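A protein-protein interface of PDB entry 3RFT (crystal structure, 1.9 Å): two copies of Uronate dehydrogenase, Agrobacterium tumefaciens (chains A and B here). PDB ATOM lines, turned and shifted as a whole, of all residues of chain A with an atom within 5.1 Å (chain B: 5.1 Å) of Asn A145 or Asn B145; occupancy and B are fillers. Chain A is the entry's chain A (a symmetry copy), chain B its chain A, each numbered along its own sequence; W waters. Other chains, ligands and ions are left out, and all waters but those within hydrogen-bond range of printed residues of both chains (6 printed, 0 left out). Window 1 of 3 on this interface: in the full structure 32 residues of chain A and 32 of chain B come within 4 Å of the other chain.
ND2 of Asn A145 lies close to ND2 of Asn B145.
The side-chain amide nitrogen (ND2) of Asn B145 sits at hydrogen-bond distance from the backbone carbonyl oxygen (O) of Cys B141, at 3.3 Å. The side-chain amide nitrogen (ND2) of Asn A145 is in hydrogen-bond range of the backbone carbonyl oxygen (O) of Cys A141.
Among the printed residues, pairs that only touch across the chains: Asn A145 with Cys B141 (3.3 Å), Cys A141 with Asn B145 (3.3 Å), Met A149 with Pro B132 (3.3 Å), Pro A132 with Met B149 (3.3 Å), Val A138 with Phe B142 (3.6 Å), Phe A142 with Val B138 (3.6 Å), Asn A145 with Pro B132 (3.6 Å), Pro A132 with Asn B145 (3.6 Å), Asn A145 with Val B138 (3.9 Å), Val A138 with Asn B145 (3.9 Å), Met A149 with Val B138 (3.9 Å), Val A138 with Met B149 (3.9 Å), Arg A148 with Ala B130 (3.9 Å) and Ala A130 with Arg B148 (3.9 Å).
Of the printed residues of chain B, Pro A132 touches Asn B145 (3.6 Å) and Met B149 (3.3 Å). Of the printed residues of chain B, Val A138 touches Phe B142 (3.6 Å), Asn B145 (3.9 Å) and Met B149 (3.9 Å). Of the printed residues of chain B, Cys A141 touches Asn B145. Printed residues of chain B within 4 Å of Phe A142: Val B138. Of the printed residues of chain B, Asn A145 touches Pro B132 (3.6 Å), Val B138 (3.9 Å), Cys B141 (3.3 Å) and Asn B145 (3.2 Å). Of the printed residues of chain A, Asn B145 touches Pro A132, Val A138, Cys A141 and Asn A145. Of the printed residues of chain A, Met B149 touches Pro A132 and Val A138. The nearest printed residue of chain B that does not touch Asn A145 is Ala B130 (4.001 Å). The nearest printed residue of chain A that does not touch Asn B145 is Ala A130 (4.0005 Å). The nearest printed residue of chain A that does not touch Pro B132 is Arg A148 (4.6 Å).
Of the 12 printed residues of chain A, 8 touch a printed residue of chain B. Hydrophobic or aromatic side chains of chain A that line the printed part of chain B: Pro A132, Val A138, Phe A142 and Met A149. Printed residues of chain B that touch a printed residue of chain A: Ala B130, Pro B132, Val B138, Cys B141, Phe B142, Asn B145, Arg B148 and Met B149. Hydrophobic or aromatic side chains of chain B within 4 Å of the printed part of chain A: Pro B132, Val B138, Phe B142 and Met B149. Along chain B the printed residues that touch a printed residue of chain A span positions 130 to 149. Among the printed residues, no Asp or Glu carboxylate lies within 4 Å of a Lys or Arg side-chain nitrogen of the other chain.
Ala A130 touches Arg B148, and with the chains exchanged Arg A148 touches Ala B130. Val A138 touches Phe B142, and with the chains exchanged Phe A142 touches Val B138. Val A138 touches Met B149, and with the chains exchanged Met A149 touches Val B138. Asn B145 touches its own counterpart, Asn A145. Positions printed for both chains: 130, 132, 138, 141, 142, 143, 144, 145, 146, 147, 148 and 149.
Water W4 lies within hydrogen-bond range of ND2 of Asn A145 (2.9 Å), O of Val B138 (3.2 Å) and N of Phe B142 (3.3 Å). Water W3 lies within hydrogen-bond range of ND2 of Asn B145, O of Val A138 and N of Phe A142. Water W5 lies within hydrogen-bond range of O of Pro A132 (2.9 Å) and O of Arg B148 (3.4 Å). Water W6 bridges O of Pro B132 and O of Arg A148. Water W2 lies within hydrogen-bond range of OD1 of Asn A145 (2.9 Å) and O of Ala B130 (2.9 Å). Water W1 lies within hydrogen-bond range of the side-chain amide oxygen (OD1) of Asn B145 and the backbone carbonyl oxygen (O) of Ala A130.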
ATOM      1  N   ALA A 130       3.106 -22.859  15.834  1.00  0.00           N
ATOM      2  CA  ALA A 130       3.860 -23.096  14.605  1.00  0.00           C
ATOM      3  C   ALA A 130       5.031 -24.050  14.862  1.00  0.00           C
ATOM      4  O   ALA A 130       5.656 -24.013  15.923  1.00  0.00           O
ATOM      5  CB  ALA A 130       4.372 -21.772  14.038  1.00  0.00           C
ATOM      6  N   PRO A 132       7.659 -24.596  12.109  1.00  0.00           N
ATOM      7  CA  PRO A 132       8.115 -24.448  10.722  1.00  0.00           C
ATOM      8  C   PRO A 132       9.282 -25.396  10.404  1.00  0.00           C
ATOM      9  O   PRO A 132      10.102 -25.685  11.282  1.00  0.00           O
ATOM     10  CB  PRO A 132       8.547 -22.974  10.636  1.00  0.00           C
ATOM     11  CG  PRO A 132       8.805 -22.552  12.042  1.00  0.00           C
ATOM     12  CD  PRO A 132       7.892 -23.385  12.920  1.00  0.00           C
ATOM     13  N   VAL A 138       9.550 -20.540   8.311  1.00  0.00           N
ATOM     14  CA  VAL A 138       9.703 -19.444   9.266  1.00  0.00           C
ATOM     15  C   VAL A 138       9.260 -18.128   8.626  1.00  0.00           C
ATOM     16  O   VAL A 138       8.602 -17.300   9.264  1.00  0.00           O
ATOM     17  CB  VAL A 138      11.164 -19.321   9.773  1.00  0.00           C
ATOM     18  CG1 VAL A 138      11.356 -18.032  10.579  1.00  0.00           C
ATOM     19  CG2 VAL A 138      11.556 -20.548  10.619  1.00  0.00           C
ATOM     20  N   CYS A 141       5.552 -17.866   8.560  1.00  0.00           N
ATOM     21  CA  CYS A 141       5.090 -17.476   9.896  1.00  0.00           C
ATOM     22  C   CYS A 141       5.225 -15.968  10.076  1.00  0.00           C
ATOM     23  O   CYS A 141       4.346 -15.327  10.653  1.00  0.00           O
ATOM     24  CB  CYS A 141       5.884 -18.172  10.995  1.00  0.00           C
ATOM     25  SG  CYS A 141       5.635 -19.978  11.079  1.00  0.00           S
ATOM     26  N   PHE A 142       6.336 -15.410   9.600  1.00  0.00           N
ATOM     27  CA  PHE A 142       6.540 -13.958   9.681  1.00  0.00           C
ATOM     28  C   PHE A 142       5.401 -13.220   8.976  1.00  0.00           C
ATOM     29  O   PHE A 142       4.829 -12.274   9.524  1.00  0.00           O
ATOM     30  CB  PHE A 142       7.898 -13.543   9.089  1.00  0.00           C
ATOM     31  CG  PHE A 142       8.079 -12.043   8.986  1.00  0.00           C
ATOM     32  CD1 PHE A 142       8.620 -11.322  10.042  1.00  0.00           C
ATOM     33  CD2 PHE A 142       7.691 -11.364   7.842  1.00  0.00           C
ATOM     34  CE1 PHE A 142       8.774  -9.942   9.958  1.00  0.00           C
ATOM     35  CE2 PHE A 142       7.844  -9.975   7.748  1.00  0.00           C
ATOM     36  CZ  PHE A 142       8.388  -9.272   8.810  1.00  0.00           C
ATOM     37  N   GLY A 143       5.071 -13.647   7.762  1.00  0.00           N
ATOM     38  CA  GLY A 143       3.943 -13.065   7.051  1.00  0.00           C
ATOM     39  C   GLY A 143       2.648 -13.119   7.854  1.00  0.00           C
ATOM     40  O   GLY A 143       1.893 -12.142   7.901  1.00  0.00           O
ATOM     41  N   GLU A 144       2.376 -14.260   8.488  1.00  0.00           N
ATOM     42  CA  GLU A 144       1.168 -14.405   9.306  1.00  0.00           C
ATOM     43  C   GLU A 144       1.164 -13.458  10.504  1.00  0.00           C
ATOM     44  O   GLU A 144       0.135 -12.849  10.819  1.00  0.00           O
ATOM     45  CB  GLU A 144       1.022 -15.850   9.812  1.00  0.00           C
ATOM     46  CG  GLU A 144       0.741 -16.867   8.705  1.00  0.00           C
ATOM     47  CD  GLU A 144       0.437 -18.262   9.254  1.00  0.00           C
ATOM     48  OE1 GLU A 144       0.359 -18.432  10.490  1.00  0.00           O
ATOM     49  OE2 GLU A 144       0.265 -19.185   8.442  1.00  0.00           O
ATOM     50  N   ASN A 145       2.298 -13.369  11.194  1.00  0.00           N
ATOM     51  CA  ASN A 145       2.388 -12.530  12.388  1.00  0.00           C
ATOM     52  C   ASN A 145       2.299 -11.059  12.025  1.00  0.00           C
ATOM     53  O   ASN A 145       1.680 -10.258  12.743  1.00  0.00           O
ATOM     54  CB  ASN A 145       3.693 -12.779  13.150  1.00  0.00           C
ATOM     55  CG  ASN A 145       3.777 -14.190  13.734  1.00  0.00           C
ATOM     56  OD1 ASN A 145       2.768 -14.784  14.123  1.00  0.00           O
ATOM     57  ND2 ASN A 145       4.987 -14.721  13.801  1.00  0.00           N
ATOM     58  N   LEU A 146       2.941 -10.694  10.922  1.00  0.00           N
ATOM     59  CA  LEU A 146       2.893  -9.308  10.463  1.00  0.00           C
ATOM     60  C   LEU A 146       1.472  -8.947  10.046  1.00  0.00           C
ATOM     61  O   LEU A 146       0.961  -7.880  10.405  1.00  0.00           O
ATOM     62  CB  LEU A 146       3.857  -9.087   9.293  1.00  0.00           C
ATOM     63  CG  LEU A 146       3.990  -7.622   8.849  1.00  0.00           C
ATOM     64  CD1 LEU A 146       5.007  -6.908   9.723  1.00  0.00           C
ATOM     65  CD2 LEU A 146       4.391  -7.542   7.379  1.00  0.00           C
ATOM     66  N   ALA A 147       0.820  -9.844   9.305  1.00  0.00           N
ATOM     67  CA  ALA A 147      -0.561  -9.611   8.901  1.00  0.00           C
ATOM     68  C   ALA A 147      -1.482  -9.458  10.114  1.00  0.00           C
ATOM     69  O   ALA A 147      -2.388  -8.612  10.115  1.00  0.00           O
ATOM     70  CB  ALA A 147      -1.065 -10.728   7.982  1.00  0.00           C
ATOM     71  N   ARG A 148      -1.280 -10.289  11.135  1.00  0.00           N
ATOM     72  CA  ARG A 148      -2.119 -10.195  12.337  1.00  0.00           C
ATOM     73  C   ARG A 148      -1.941  -8.841  13.007  1.00  0.00           C
ATOM     74  O   ARG A 148      -2.908  -8.248  13.492  1.00  0.00           O
ATOM     75  CB  ARG A 148      -1.785 -11.303  13.342  1.00  0.00           C
ATOM     76  CG  ARG A 148      -2.636 -11.247  14.630  1.00  0.00           C
ATOM     77  CD  ARG A 148      -4.113 -11.582  14.360  1.00  0.00           C
ATOM     78  NE  ARG A 148      -5.017 -10.917  15.301  1.00  0.00           N
ATOM     79  CZ  ARG A 148      -6.269 -11.295  15.540  1.00  0.00           C
ATOM     80  NH1 ARG A 148      -6.777 -12.367  14.931  1.00  0.00           N
ATOM     81  NH2 ARG A 148      -7.013 -10.608  16.401  1.00  0.00           N
ATOM     82  N   MET A 149      -0.700  -8.369  13.061  1.00  0.00           N
ATOM     83  CA  MET A 149      -0.420  -7.069  13.675  1.00  0.00           C
ATOM     84  C   MET A 149      -1.113  -5.927  12.921  1.00  0.00           C
ATOM     85  O   MET A 149      -1.707  -5.035  13.541  1.00  0.00           O
ATOM     86  CB  MET A 149       1.095  -6.827  13.781  1.00  0.00           C
ATOM     87  CG  MET A 149       1.483  -5.552  14.533  1.00  0.00           C
ATOM     88  SD  MET A 149       1.577  -4.103  13.443  1.00  0.00           S
ATOM     89  CE  MET A 149       3.104  -4.441  12.553  1.00  0.00           C
ATOM     90  N   ALA B 130      -0.062 -15.825  18.645  1.00  0.00           N
ATOM     91  CA  ALA B 130       0.594 -14.531  18.815  1.00  0.00           C
ATOM     92  C   ALA B 130      -0.332 -13.392  18.373  1.00  0.00           C
ATOM     93  O   ALA B 130      -1.093 -13.531  17.414  1.00  0.00           O
ATOM     94  CB  ALA B 130       1.896 -14.491  18.017  1.00  0.00           C
ATOM     95  N   PRO B 132       1.068  -9.822  18.098  1.00  0.00           N
ATOM     96  CA  PRO B 132       2.124  -8.834  18.348  1.00  0.00           C
ATOM     97  C   PRO B 132       1.610  -7.396  18.176  1.00  0.00           C
ATOM     98  O   PRO B 132       0.737  -7.148  17.338  1.00  0.00           O
ATOM     99  CB  PRO B 132       3.199  -9.177  17.302  1.00  0.00           C
ATOM    100  CG  PRO B 132       2.489  -9.939  16.236  1.00  0.00           C
ATOM    101  CD  PRO B 132       1.336 -10.657  16.911  1.00  0.00           C
ATOM    102  N   VAL B 138       6.498  -8.382  16.394  1.00  0.00           N
ATOM    103  CA  VAL B 138       6.587  -9.296  15.257  1.00  0.00           C
ATOM    104  C   VAL B 138       7.994  -9.888  15.172  1.00  0.00           C
ATOM    105  O   VAL B 138       8.167 -11.081  14.899  1.00  0.00           O
ATOM    106  CB  VAL B 138       6.228  -8.592  13.922  1.00  0.00           C
ATOM    107  CG1 VAL B 138       6.556  -9.490  12.725  1.00  0.00           C
ATOM    108  CG2 VAL B 138       4.741  -8.187  13.898  1.00  0.00           C
ATOM    109  N   CYS B 141       8.450 -12.592  17.683  1.00  0.00           N
ATOM    110  CA  CYS B 141       7.809 -13.810  17.176  1.00  0.00           C
ATOM    111  C   CYS B 141       8.738 -14.519  16.196  1.00  0.00           C
ATOM    112  O   CYS B 141       8.836 -15.747  16.207  1.00  0.00           O
ATOM    113  CB  CYS B 141       6.494 -13.505  16.468  1.00  0.00           C
ATOM    114  SG  CYS B 141       5.175 -12.876  17.563  1.00  0.00           S
ATOM    115  N   PHE B 142       9.401 -13.745  15.339  1.00  0.00           N
ATOM    116  CA  PHE B 142      10.355 -14.328  14.387  1.00  0.00           C
ATOM    117  C   PHE B 142      11.442 -15.104  15.131  1.00  0.00           C
ATOM    118  O   PHE B 142      11.756 -16.244  14.777  1.00  0.00           O
ATOM    119  CB  PHE B 142      10.984 -13.251  13.486  1.00  0.00           C
ATOM    120  CG  PHE B 142      12.104 -13.775  12.611  1.00  0.00           C
ATOM    121  CD1 PHE B 142      11.834 -14.292  11.351  1.00  0.00           C
ATOM    122  CD2 PHE B 142      13.414 -13.762  13.062  1.00  0.00           C
ATOM    123  CE1 PHE B 142      12.857 -14.788  10.550  1.00  0.00           C
ATOM    124  CE2 PHE B 142      14.451 -14.257  12.262  1.00  0.00           C
ATOM    125  CZ  PHE B 142      14.165 -14.767  11.006  1.00  0.00           C
ATOM    126  N   GLY B 143      12.019 -14.493  16.160  1.00  0.00           N
ATOM    127  CA  GLY B 143      12.999 -15.186  16.982  1.00  0.00           C
ATOM    128  C   GLY B 143      12.472 -16.500  17.548  1.00  0.00           C
ATOM    129  O   GLY B 143      13.173 -17.516  17.542  1.00  0.00           O
ATOM    130  N   GLU B 144      11.236 -16.490  18.048  1.00  0.00           N
ATOM    131  CA  GLU B 144      10.629 -17.708  18.594  1.00  0.00           C
ATOM    132  C   GLU B 144      10.450 -18.791  17.533  1.00  0.00           C
ATOM    133  O   GLU B 144      10.721 -19.971  17.789  1.00  0.00           O
ATOM    134  CB  GLU B 144       9.261 -17.400  19.225  1.00  0.00           C
ATOM    135  CG  GLU B 144       9.343 -16.533  20.483  1.00  0.00           C
ATOM    136  CD  GLU B 144       7.989 -16.382  21.180  1.00  0.00           C
ATOM    137  OE1 GLU B 144       7.001 -17.012  20.745  1.00  0.00           O
ATOM    138  OE2 GLU B 144       7.922 -15.638  22.171  1.00  0.00           O
ATOM    139  N   ASN B 145       9.958 -18.399  16.361  1.00  0.00           N
ATOM    140  CA  ASN B 145       9.701 -19.363  15.293  1.00  0.00           C
ATOM    141  C   ASN B 145      11.001 -19.926  14.746  1.00  0.00           C
ATOM    142  O   ASN B 145      11.096 -21.120  14.421  1.00  0.00           O
ATOM    143  CB  ASN B 145       8.909 -18.730  14.145  1.00  0.00           C
ATOM    144  CG  ASN B 145       7.496 -18.316  14.560  1.00  0.00           C
ATOM    145  OD1 ASN B 145       6.863 -18.956  15.405  1.00  0.00           O
ATOM    146  ND2 ASN B 145       7.001 -17.249  13.956  1.00  0.00           N
ATOM    147  N   LEU B 146      11.998 -19.060  14.617  1.00  0.00           N
ATOM    148  CA  LEU B 146      13.303 -19.503  14.131  1.00  0.00           C
ATOM    149  C   LEU B 146      13.938 -20.454  15.139  1.00  0.00           C
ATOM    150  O   LEU B 146      14.468 -21.506  14.765  1.00  0.00           O
ATOM    151  CB  LEU B 146      14.227 -18.307  13.882  1.00  0.00           C
ATOM    152  CG  LEU B 146      15.566 -18.666  13.219  1.00  0.00           C
ATOM    153  CD1 LEU B 146      15.391 -18.748  11.713  1.00  0.00           C
ATOM    154  CD2 LEU B 146      16.636 -17.641  13.584  1.00  0.00           C
ATOM    155  N   ALA B 147      13.868 -20.099  16.422  1.00  0.00           N
ATOM    156  CA  ALA B 147      14.401 -20.968  17.464  1.00  0.00           C
ATOM    157  C   ALA B 147      13.708 -22.333  17.463  1.00  0.00           C
ATOM    158  O   ALA B 147      14.359 -23.371  17.654  1.00  0.00           O
ATOM    159  CB  ALA B 147      14.293 -20.311  18.843  1.00  0.00           C
ATOM    160  N   ARG B 148      12.389 -22.341  17.282  1.00  0.00           N
ATOM    161  CA  ARG B 148      11.656 -23.614  17.261  1.00  0.00           C
ATOM    162  C   ARG B 148      12.128 -24.481  16.104  1.00  0.00           C
ATOM    163  O   ARG B 148      12.262 -25.699  16.245  1.00  0.00           O
ATOM    164  CB  ARG B 148      10.145 -23.390  17.141  1.00  0.00           C
ATOM    165  CG  ARG B 148       9.327 -24.700  17.108  1.00  0.00           C
ATOM    166  CD  ARG B 148       9.370 -25.441  18.456  1.00  0.00           C
ATOM    167  NE  ARG B 148       9.229 -26.890  18.300  1.00  0.00           N
ATOM    168  CZ  ARG B 148       8.869 -27.722  19.272  1.00  0.00           C
ATOM    169  NH1 ARG B 148       8.574 -27.254  20.485  1.00  0.00           N
ATOM    170  NH2 ARG B 148       8.791 -29.027  19.030  1.00  0.00           N
ATOM    171  N   MET B 149      12.347 -23.856  14.951  1.00  0.00           N
ATOM    172  CA  MET B 149      12.814 -24.596  13.776  1.00  0.00           C
ATOM    173  C   MET B 149      14.194 -25.222  14.014  1.00  0.00           C
ATOM    174  O   MET B 149      14.421 -26.390  13.670  1.00  0.00           O
ATOM    175  CB  MET B 149      12.819 -23.697  12.529  1.00  0.00           C
ATOM    176  CG  MET B 149      13.164 -24.422  11.225  1.00  0.00           C
ATOM    177  SD  MET B 149      14.950 -24.460  10.903  1.00  0.00           S
ATOM    178  CE  MET B 149      15.247 -22.751  10.421  1.00  0.00           C
HETATM  179  O   HOH W   1       7.161 -21.593  16.544  1.00  0.00           O
HETATM  180  O   HOH W   2       0.085 -13.937  14.776  1.00  0.00           O
HETATM  181  O   HOH W   3       8.496 -15.752  12.027  1.00  0.00           O
HETATM  182  O   HOH W   4       7.315 -13.347  12.856  1.00  0.00           O
HETATM  183  O   HOH W   5       9.639 -26.093  14.096  1.00  0.00           O
HETATM  184  O   HOH W   6      -1.511  -8.774  16.561  1.00  0.00           O
